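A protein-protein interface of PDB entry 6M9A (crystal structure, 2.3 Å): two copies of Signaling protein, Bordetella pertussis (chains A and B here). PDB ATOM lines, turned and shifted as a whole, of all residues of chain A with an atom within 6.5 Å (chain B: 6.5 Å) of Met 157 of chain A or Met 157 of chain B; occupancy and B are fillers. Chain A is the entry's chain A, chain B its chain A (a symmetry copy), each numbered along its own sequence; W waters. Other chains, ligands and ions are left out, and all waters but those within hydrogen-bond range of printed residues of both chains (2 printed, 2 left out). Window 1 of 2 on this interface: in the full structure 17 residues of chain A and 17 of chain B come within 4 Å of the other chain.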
ATOM      1  N   VAL A 119      23.624 -22.181   7.502  1.00  0.00           N
ATOM      2  CA  VAL A 119      22.469 -21.290   7.368  1.00  0.00           C
ATOM      3  C   VAL A 119      22.479 -20.221   8.460  1.00  0.00           C
ATOM      4  O   VAL A 119      22.249 -19.035   8.194  1.00  0.00           O
ATOM      5  CB  VAL A 119      21.170 -22.116   7.390  1.00  0.00           C
ATOM      6  CG1 VAL A 119      19.971 -21.206   7.363  1.00  0.00           C
ATOM      7  CG2 VAL A 119      21.145 -23.100   6.197  1.00  0.00           C
ATOM      8  N   THR A 120      22.745 -20.628   9.705  1.00  0.00           N
ATOM      9  CA  THR A 120      22.903 -19.673  10.801  1.00  0.00           C
ATOM     10  C   THR A 120      23.986 -18.651  10.488  1.00  0.00           C
ATOM     11  O   THR A 120      23.776 -17.438  10.631  1.00  0.00           O
ATOM     12  CB  THR A 120      23.247 -20.429  12.086  1.00  0.00           C
ATOM     13  OG1 THR A 120      22.085 -21.122  12.544  1.00  0.00           O
ATOM     14  CG2 THR A 120      23.770 -19.491  13.158  1.00  0.00           C
ATOM     15  N   ARG A 121      25.167 -19.138  10.073  1.00  0.00           N
ATOM     16  CA  ARG A 121      26.286 -18.253   9.784  1.00  0.00           C
ATOM     17  C   ARG A 121      25.925 -17.254   8.695  1.00  0.00           C
ATOM     18  O   ARG A 121      26.294 -16.077   8.776  1.00  0.00           O
ATOM     19  CB  ARG A 121      27.523 -19.066   9.368  1.00  0.00           C
ATOM     20  CG  ARG A 121      28.737 -18.166   9.004  1.00  0.00           C
ATOM     21  CD  ARG A 121      29.835 -18.904   8.233  1.00  0.00           C
ATOM     22  NE  ARG A 121      30.239 -20.117   8.935  1.00  0.00           N
ATOM     23  CZ  ARG A 121      31.074 -21.036   8.459  1.00  0.00           C
ATOM     24  NH1 ARG A 121      31.611 -20.900   7.254  1.00  0.00           N
ATOM     25  NH2 ARG A 121      31.367 -22.099   9.196  1.00  0.00           N
ATOM     26  N   ALA A 123      22.865 -16.115   7.891  1.00  0.00           N
ATOM     27  CA  ALA A 123      21.992 -15.126   8.520  1.00  0.00           C
ATOM     28  C   ALA A 123      22.797 -14.093   9.302  1.00  0.00           C
ATOM     29  O   ALA A 123      22.565 -12.883   9.185  1.00  0.00           O
ATOM     30  CB  ALA A 123      21.004 -15.832   9.438  1.00  0.00           C
ATOM     31  N   CYS A 124      23.756 -14.565  10.102  1.00  0.00           N
ATOM     32  CA  CYS A 124      24.622 -13.670  10.865  1.00  0.00           C
ATOM     33  C   CYS A 124      25.384 -12.710   9.945  1.00  0.00           C
ATOM     34  O   CYS A 124      25.533 -11.524  10.262  1.00  0.00           O
ATOM     35  CB  CYS A 124      25.582 -14.514  11.709  1.00  0.00           C
ATOM     36  SG  CYS A 124      26.895 -13.646  12.601  1.00  0.00           S
ATOM     37  N   ILE A 127      22.933 -10.010   8.790  1.00  0.00           N
ATOM     38  CA  ILE A 127      22.584  -9.072   9.856  1.00  0.00           C
ATOM     39  C   ILE A 127      23.707  -8.057  10.057  1.00  0.00           C
ATOM     40  O   ILE A 127      23.472  -6.845  10.153  1.00  0.00           O
ATOM     41  CB  ILE A 127      22.268  -9.835  11.158  1.00  0.00           C
ATOM     42  CG1 ILE A 127      20.946 -10.612  11.031  1.00  0.00           C
ATOM     43  CG2 ILE A 127      22.214  -8.853  12.327  1.00  0.00           C
ATOM     44  CD1 ILE A 127      20.638 -11.603  12.233  1.00  0.00           C
ATOM     45  N   VAL A 152      16.240  -5.413  12.591  1.00  0.00           N
ATOM     46  CA  VAL A 152      16.885  -6.161  11.521  1.00  0.00           C
ATOM     47  C   VAL A 152      17.245  -7.562  11.995  1.00  0.00           C
ATOM     48  O   VAL A 152      16.897  -8.548  11.352  1.00  0.00           O
ATOM     49  CB  VAL A 152      18.156  -5.454  11.015  1.00  0.00           C
ATOM     50  CG1 VAL A 152      19.072  -6.448  10.321  1.00  0.00           C
ATOM     51  CG2 VAL A 152      17.790  -4.317  10.073  1.00  0.00           C
ATOM     52  N   ALA A 153      17.934  -7.641  13.127  1.00  0.00           N
ATOM     53  CA  ALA A 153      18.336  -8.925  13.690  1.00  0.00           C
ATOM     54  C   ALA A 153      17.120  -9.774  14.043  1.00  0.00           C
ATOM     55  O   ALA A 153      17.110 -10.982  13.817  1.00  0.00           O
ATOM     56  CB  ALA A 153      19.212  -8.716  14.916  1.00  0.00           C
ATOM     57  N   ASP A 154      16.097  -9.132  14.595  1.00  0.00           N
ATOM     58  CA  ASP A 154      14.872  -9.819  14.984  1.00  0.00           C
ATOM     59  C   ASP A 154      14.152 -10.445  13.792  1.00  0.00           C
ATOM     60  O   ASP A 154      13.834 -11.633  13.805  1.00  0.00           O
ATOM     61  CB  ASP A 154      13.930  -8.857  15.710  1.00  0.00           C
ATOM     62  CG  ASP A 154      13.951  -9.044  17.213  1.00  0.00           C
ATOM     63  OD1 ASP A 154      14.592 -10.007  17.685  1.00  0.00           O
ATOM     64  OD2 ASP A 154      13.329  -8.229  17.923  1.00  0.00           O
ATOM     65  N   VAL A 155      13.898  -9.641  12.764  1.00  0.00           N
ATOM     66  CA  VAL A 155      13.195 -10.123  11.577  1.00  0.00           C
ATOM     67  C   VAL A 155      14.020 -11.091  10.726  1.00  0.00           C
ATOM     68  O   VAL A 155      13.460 -11.944  10.039  1.00  0.00           O
ATOM     69  CB  VAL A 155      12.651  -8.961  10.715  1.00  0.00           C
ATOM     70  CG1 VAL A 155      13.777  -8.226  10.004  1.00  0.00           C
ATOM     71  CG2 VAL A 155      11.618  -9.472   9.723  1.00  0.00           C
ATOM     72  N   THR A 156      15.343 -10.964  10.773  1.00  0.00           N
ATOM     73  CA  THR A 156      16.206 -11.855  10.006  1.00  0.00           C
ATOM     74  C   THR A 156      16.245 -13.216  10.684  1.00  0.00           C
ATOM     75  O   THR A 156      16.155 -14.250  10.027  1.00  0.00           O
ATOM     76  CB  THR A 156      17.638 -11.307   9.871  1.00  0.00           C
ATOM     77  OG1 THR A 156      17.597  -9.990   9.307  1.00  0.00           O
ATOM     78  CG2 THR A 156      18.470 -12.209   8.974  1.00  0.00           C
ATOM     79  N   MET A 157      16.366 -13.204  12.008  1.00  0.00           N
ATOM     80  CA  MET A 157      16.393 -14.437  12.784  1.00  0.00           C
ATOM     81  C   MET A 157      15.037 -15.124  12.690  1.00  0.00           C
ATOM     82  O   MET A 157      14.956 -16.348  12.596  1.00  0.00           O
ATOM     83  CB  MET A 157      16.742 -14.150  14.244  1.00  0.00           C
ATOM     84  CG  MET A 157      18.225 -13.926  14.493  1.00  0.00           C
ATOM     85  SD  MET A 157      19.206 -15.412  14.217  1.00  0.00           S
ATOM     86  CE  MET A 157      19.333 -15.408  12.432  1.00  0.00           C
ATOM     87  N   THR A 158      13.973 -14.326  12.721  1.00  0.00           N
ATOM     88  CA  THR A 158      12.623 -14.854  12.613  1.00  0.00           C
ATOM     89  C   THR A 158      12.502 -15.644  11.318  1.00  0.00           C
ATOM     90  O   THR A 158      11.978 -16.757  11.309  1.00  0.00           O
ATOM     91  CB  THR A 158      11.571 -13.732  12.631  1.00  0.00           C
ATOM     92  OG1 THR A 158      11.487 -13.174  13.947  1.00  0.00           O
ATOM     93  CG2 THR A 158      10.209 -14.274  12.228  1.00  0.00           C
ATOM     94  N   ALA A 159      12.990 -15.068  10.221  1.00  0.00           N
ATOM     95  CA  ALA A 159      12.937 -15.757   8.934  1.00  0.00           C
ATOM     96  C   ALA A 159      13.761 -17.047   8.965  1.00  0.00           C
ATOM     97  O   ALA A 159      13.321 -18.089   8.451  1.00  0.00           O
ATOM     98  CB  ALA A 159      13.403 -14.813   7.818  1.00  0.00           C
ATOM     99  N   VAL A 160      14.935 -17.013   9.606  1.00  0.00           N
ATOM    100  CA  VAL A 160      15.784 -18.203   9.682  1.00  0.00           C
ATOM    101  C   VAL A 160      15.145 -19.275  10.557  1.00  0.00           C
ATOM    102  O   VAL A 160      15.258 -20.474  10.274  1.00  0.00           O
ATOM    103  CB  VAL A 160      17.192 -17.810  10.169  1.00  0.00           C
ATOM    104  CG1 VAL A 160      18.069 -19.024  10.337  1.00  0.00           C
ATOM    105  CG2 VAL A 160      17.797 -16.880   9.162  1.00  0.00           C
ATOM    106  N   GLU A 161      14.459 -18.869  11.624  1.00  0.00           N
ATOM    107  CA  GLU A 161      13.746 -19.847  12.433  1.00  0.00           C
ATOM    108  C   GLU A 161      12.721 -20.610  11.598  1.00  0.00           C
ATOM    109  O   GLU A 161      12.610 -21.836  11.705  1.00  0.00           O
ATOM    110  CB  GLU A 161      13.058 -19.166  13.611  1.00  0.00           C
ATOM    111  CG  GLU A 161      12.302 -20.160  14.483  1.00  0.00           C
ATOM    112  CD  GLU A 161      11.461 -19.487  15.541  1.00  0.00           C
ATOM    113  OE1 GLU A 161      11.851 -18.393  15.998  1.00  0.00           O
ATOM    114  OE2 GLU A 161      10.401 -20.043  15.900  1.00  0.00           O
ATOM    115  N   MET A 162      11.959 -19.893  10.764  1.00  0.00           N
ATOM    116  CA  MET A 162      10.987 -20.538   9.888  1.00  0.00           C
ATOM    117  C   MET A 162      11.672 -21.436   8.861  1.00  0.00           C
ATOM    118  O   MET A 162      11.197 -22.538   8.590  1.00  0.00           O
ATOM    119  CB  MET A 162      10.148 -19.487   9.169  1.00  0.00           C
ATOM    120  CG  MET A 162       9.629 -18.356  10.037  1.00  0.00           C
ATOM    121  SD  MET A 162       8.135 -18.796  10.912  1.00  0.00           S
ATOM    122  CE  MET A 162       7.586 -17.176  11.430  1.00  0.00           C
ATOM    123  N   VAL B 119      16.501 -23.271  19.456  1.00  0.00           N
ATOM    124  CA  VAL B 119      17.823 -22.755  19.818  1.00  0.00           C
ATOM    125  C   VAL B 119      18.099 -21.428  19.115  1.00  0.00           C
ATOM    126  O   VAL B 119      18.585 -20.469  19.729  1.00  0.00           O
ATOM    127  CB  VAL B 119      18.898 -23.809  19.491  1.00  0.00           C
ATOM    128  CG1 VAL B 119      20.272 -23.253  19.756  1.00  0.00           C
ATOM    129  CG2 VAL B 119      18.653 -25.094  20.316  1.00  0.00           C
ATOM    130  N   THR B 120      17.793 -21.354  17.815  1.00  0.00           N
ATOM    131  CA  THR B 120      17.899 -20.095  17.079  1.00  0.00           C
ATOM    132  C   THR B 120      17.068 -19.002  17.735  1.00  0.00           C
ATOM    133  O   THR B 120      17.555 -17.887  17.970  1.00  0.00           O
ATOM    134  CB  THR B 120      17.439 -20.312  15.636  1.00  0.00           C
ATOM    135  OG1 THR B 120      18.427 -21.074  14.942  1.00  0.00           O
ATOM    136  CG2 THR B 120      17.185 -18.993  14.930  1.00  0.00           C
ATOM    137  N   ARG B 121      15.793 -19.310  18.021  1.00  0.00           N
ATOM    138  CA  ARG B 121      14.896 -18.328  18.613  1.00  0.00           C
ATOM    139  C   ARG B 121      15.435 -17.829  19.945  1.00  0.00           C
ATOM    140  O   ARG B 121      15.349 -16.633  20.249  1.00  0.00           O
ATOM    141  CB  ARG B 121      13.491 -18.924  18.801  1.00  0.00           C
ATOM    142  CG  ARG B 121      12.503 -17.929  19.472  1.00  0.00           C
ATOM    143  CD  ARG B 121      11.237 -18.598  20.015  1.00  0.00           C
ATOM    144  NE  ARG B 121      10.592 -19.405  18.985  1.00  0.00           N
ATOM    145  CZ  ARG B 121       9.552 -20.210  19.181  1.00  0.00           C
ATOM    146  NH1 ARG B 121       9.016 -20.337  20.387  1.00  0.00           N
ATOM    147  NH2 ARG B 121       9.051 -20.893  18.161  1.00  0.00           N
ATOM    148  N   ALA B 123      18.643 -17.730  20.949  1.00  0.00           N
ATOM    149  CA  ALA B 123      19.742 -16.822  20.629  1.00  0.00           C
ATOM    150  C   ALA B 123      19.225 -15.441  20.238  1.00  0.00           C
ATOM    151  O   ALA B 123      19.723 -14.415  20.717  1.00  0.00           O
ATOM    152  CB  ALA B 123      20.576 -17.413  19.500  1.00  0.00           C
ATOM    153  N   CYS B 124      18.214 -15.407  19.367  1.00  0.00           N
ATOM    154  CA  CYS B 124      17.605 -14.146  18.954  1.00  0.00           C
ATOM    155  C   CYS B 124      17.049 -13.373  20.155  1.00  0.00           C
ATOM    156  O   CYS B 124      17.188 -12.146  20.229  1.00  0.00           O
ATOM    157  CB  CYS B 124      16.509 -14.441  17.925  1.00  0.00           C
ATOM    158  SG  CYS B 124      15.464 -13.061  17.397  1.00  0.00           S
ATOM    159  N   ILE B 127      20.009 -11.805  22.002  1.00  0.00           N
ATOM    160  CA  ILE B 127      20.602 -10.688  21.270  1.00  0.00           C
ATOM    161  C   ILE B 127      19.751  -9.432  21.438  1.00  0.00           C
ATOM    162  O   ILE B 127      20.260  -8.337  21.715  1.00  0.00           O
ATOM    163  CB  ILE B 127      20.784 -11.057  19.784  1.00  0.00           C
ATOM    164  CG1 ILE B 127      21.887 -12.116  19.613  1.00  0.00           C
ATOM    165  CG2 ILE B 127      21.105  -9.800  18.978  1.00  0.00           C
ATOM    166  CD1 ILE B 127      22.004 -12.726  18.152  1.00  0.00           C
ATOM    167  N   VAL B 152      27.714  -7.914  19.578  1.00  0.00           N
ATOM    168  CA  VAL B 152      26.875  -8.790  20.385  1.00  0.00           C
ATOM    169  C   VAL B 152      26.222  -9.851  19.512  1.00  0.00           C
ATOM    170  O   VAL B 152      26.310 -11.041  19.801  1.00  0.00           O
ATOM    171  CB  VAL B 152      25.782  -8.005  21.133  1.00  0.00           C
ATOM    172  CG1 VAL B 152      24.637  -8.928  21.516  1.00  0.00           C
ATOM    173  CG2 VAL B 152      26.364  -7.334  22.368  1.00  0.00           C
ATOM    174  N   ALA B 153      25.575  -9.413  18.437  1.00  0.00           N
ATOM    175  CA  ALA B 153      24.911 -10.329  17.518  1.00  0.00           C
ATOM    176  C   ALA B 153      25.913 -11.282  16.873  1.00  0.00           C
ATOM    177  O   ALA B 153      25.637 -12.468  16.711  1.00  0.00           O
ATOM    178  CB  ALA B 153      24.153  -9.554  16.452  1.00  0.00           C
ATOM    179  N   ASP B 154      27.075 -10.751  16.511  1.00  0.00           N
ATOM    180  CA  ASP B 154      28.124 -11.545  15.882  1.00  0.00           C
ATOM    181  C   ASP B 154      28.637 -12.658  16.791  1.00  0.00           C
ATOM    182  O   ASP B 154      28.674 -13.823  16.397  1.00  0.00           O
ATOM    183  CB  ASP B 154      29.288 -10.646  15.457  1.00  0.00           C
ATOM    184  CG  ASP B 154      29.280 -10.346  13.973  1.00  0.00           C
ATOM    185  OD1 ASP B 154      28.454 -10.939  13.248  1.00  0.00           O
ATOM    186  OD2 ASP B 154      30.099  -9.515  13.530  1.00  0.00           O
ATOM    187  N   VAL B 155      29.029 -12.295  18.009  1.00  0.00           N
ATOM    188  CA  VAL B 155      29.559 -13.271  18.959  1.00  0.00           C
ATOM    189  C   VAL B 155      28.503 -14.240  19.496  1.00  0.00           C
ATOM    190  O   VAL B 155      28.826 -15.369  19.861  1.00  0.00           O
ATOM    191  CB  VAL B 155      30.322 -12.593  20.119  1.00  0.00           C
ATOM    192  CG1 VAL B 155      29.369 -11.879  21.066  1.00  0.00           C
ATOM    193  CG2 VAL B 155      31.173 -13.610  20.864  1.00  0.00           C
ATOM    194  N   THR B 156      27.247 -13.805  19.540  1.00  0.00           N
ATOM    195  CA  THR B 156      26.174 -14.668  20.022  1.00  0.00           C
ATOM    196  C   THR B 156      25.851 -15.703  18.956  1.00  0.00           C
ATOM    197  O   THR B 156      25.676 -16.882  19.254  1.00  0.00           O
ATOM    198  CB  THR B 156      24.902 -13.877  20.375  1.00  0.00           C
ATOM    199  OG1 THR B 156      25.223 -12.848  21.320  1.00  0.00           O
ATOM    200  CG2 THR B 156      23.853 -14.798  20.976  1.00  0.00           C
ATOM    201  N   MET B 157      25.784 -15.251  17.707  1.00  0.00           N
ATOM    202  CA  MET B 157      25.504 -16.140  16.587  1.00  0.00           C
ATOM    203  C   MET B 157      26.663 -17.114  16.412  1.00  0.00           C
ATOM    204  O   MET B 157      26.458 -18.290  16.116  1.00  0.00           O
ATOM    205  CB  MET B 157      25.285 -15.340  15.303  1.00  0.00           C
ATOM    206  CG  MET B 157      23.903 -14.716  15.191  1.00  0.00           C
ATOM    207  SD  MET B 157      22.598 -15.948  15.027  1.00  0.00           S
ATOM    208  CE  MET B 157      22.410 -16.471  16.728  1.00  0.00           C
ATOM    209  N   THR B 158      27.881 -16.612  16.591  1.00  0.00           N
ATOM    210  CA  THR B 158      29.069 -17.441  16.480  1.00  0.00           C
ATOM    211  C   THR B 158      28.958 -18.602  17.458  1.00  0.00           C
ATOM    212  O   THR B 158      29.213 -19.751  17.100  1.00  0.00           O
ATOM    213  CB  THR B 158      30.351 -16.643  16.773  1.00  0.00           C
ATOM    214  OG1 THR B 158      30.610 -15.737  15.694  1.00  0.00           O
ATOM    215  CG2 THR B 158      31.537 -17.580  16.936  1.00  0.00           C
ATOM    216  N   ALA B 159      28.575 -18.301  18.697  1.00  0.00           N
ATOM    217  CA  ALA B 159      28.421 -19.349  19.702  1.00  0.00           C
ATOM    218  C   ALA B 159      27.324 -20.341  19.301  1.00  0.00           C
ATOM    219  O   ALA B 159      27.495 -21.562  19.447  1.00  0.00           O
ATOM    220  CB  ALA B 159      28.142 -18.720  21.073  1.00  0.00           C
ATOM    221  N   VAL B 160      26.214 -19.840  18.747  1.00  0.00           N
ATOM    222  CA  VAL B 160      25.119 -20.719  18.335  1.00  0.00           C
ATOM    223  C   VAL B 160      25.527 -21.582  17.146  1.00  0.00           C
ATOM    224  O   VAL B 160      25.132 -22.750  17.046  1.00  0.00           O
ATOM    225  CB  VAL B 160      23.857 -19.882  18.047  1.00  0.00           C
ATOM    226  CG1 VAL B 160      22.733 -20.749  17.542  1.00  0.00           C
ATOM    227  CG2 VAL B 160      23.445 -19.201  19.316  1.00  0.00           C
ATOM    228  N   GLU B 161      26.328 -21.031  16.234  1.00  0.00           N
ATOM    229  CA  GLU B 161      26.827 -21.845  15.134  1.00  0.00           C
ATOM    230  C   GLU B 161      27.618 -23.043  15.652  1.00  0.00           C
ATOM    231  O   GLU B 161      27.449 -24.166  15.163  1.00  0.00           O
ATOM    232  CB  GLU B 161      27.696 -21.007  14.203  1.00  0.00           C
ATOM    233  CG  GLU B 161      28.236 -21.825  13.037  1.00  0.00           C
ATOM    234  CD  GLU B 161      29.247 -21.066  12.211  1.00  0.00           C
ATOM    235  OE1 GLU B 161      29.136 -19.827  12.133  1.00  0.00           O
ATOM    236  OE2 GLU B 161      30.164 -21.710  11.658  1.00  0.00           O
ATOM    237  N   MET B 162      28.492 -22.817  16.638  1.00  0.00           N
ATOM    238  CA  MET B 162      29.258 -23.907  17.233  1.00  0.00           C
ATOM    239  C   MET B 162      28.347 -24.899  17.953  1.00  0.00           C
ATOM    240  O   MET B 162      28.546 -26.108  17.849  1.00  0.00           O
ATOM    241  CB  MET B 162      30.288 -23.354  18.212  1.00  0.00           C
ATOM    242  CG  MET B 162      31.084 -22.160  17.722  1.00  0.00           C
ATOM    243  SD  MET B 162      32.468 -22.635  16.698  1.00  0.00           S
ATOM    244  CE  MET B 162      33.393 -21.105  16.691  1.00  0.00           C
HETATM  245  O   HOH W   1      17.414 -10.352  17.824  1.00  0.00           O
HETATM  246  O   HOH W   2      25.635 -10.567  13.114  1.00  0.00           O
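Printed residues of chain A that touch a printed residue of chain B: Arg 121, Cys 124, Asp 154, Met 157 and Glu 161. Hydrophobic or aromatic side chains of chain A that line the printed part of chain B: Met 157. Among the printed residues, Asp or Glu carboxylates within 4 Å of a Lys or Arg side-chain nitrogen of the other chain: Arg 121 of chain A with Glu 161 of chain B and Glu 161 of chain A with Arg 121 of chain B.
Arg 121 of chain A touches Glu 161 of chain B, and with the chains exchanged Glu 161 of chain A touches Arg 121 of chain B. Cys 124 of chain A touches Asp 154 of chain B, and with the chains exchanged Asp 154 of chain A touches Cys 124 of chain B. Cys 124 of chain A touches Met 157 of chain B, and with the chains exchanged Met 157 of chain A touches Cys 124 of chain B. Met 157 of chain A touches its own counterpart, Met 157 of chain B. Of the 7 pairs that touch across the chains among the printed residues, 7 have their exchanged pair printed and touching as well.
Water W2 bridges the side-chain carboxylate (OD1) of Asp 154 of chain B (2.8 Å) and the backbone carbonyl oxygen (O) of Cys 124 of chain A (3.0 Å). Water W1 bridges OD1 of Asp 154 of chain A (2.8 Å) and O of Cys 124 of chain B (3.0 Å).
Printed residues of chain B within 4 Å of Arg 121 of chain A: Glu 161. Printed residues of chain B within 4 Å of Cys 124 of chain A: Asp 154 (3.2 Å) and Met 157 (3.6 Å). Ala 153 of chain A touches none of the printed residues of chain B. Of the printed residues of chain B, Asp 154 of chain A touches Cys 124. Thr 156 of chain A touches none of the printed residues of chain B. Printed residues of chain B within 4 Å of Glu 161 of chain A: Arg 121 (2.8 Å). Of the printed residues of chain A, Arg 121 of chain B touches Glu 161 (2.8 Å). Met 157 of chain B touches two residues of chain A. The nearest printed residue of chain A that does not touch Asp 154 of chain B is Ile 127 of chain A (6.4 Å).
Cys 124 of chain A touches Met 157 of chain B. SG of Cys 124 of chain B touches CB of Met 157 of chain A, at 3.6 Å.
The guanidinium group (NH2) of Arg 121 of chain A lies within salt-bridge range of the side-chain carboxylate (OE2) of Glu 161 of chain B. The side-chain carboxylate (OD1) of Asp 154 of chain B sits at hydrogen-bond distance from the side-chain sulfur (SG) of Cys 124 of chain A (3.2 Å). The side-chain carboxylate (OD1) of Asp 154 of chain A lies within hydrogen-bond range of the side-chain sulfur (SG) of Cys 124 of chain B. OE2 of Glu 161 of chain A is in salt-bridge range of NH2 of Arg 121 of chain B (2.8 Å). The side-chain sulfur (SD) of Met 157 of chain A lies close to the side-chain sulfur (SD) of Met 157 of chain B.
O of Asp 154 of chain A sits at hydrogen-bond distance from OG1 of Thr 158 of chain A. The side-chain hydroxyl of Thr 158 of chain B lies within hydrogen-bond range of the backbone carbonyl oxygen of Asp 154 of chain B (2.8 Å).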
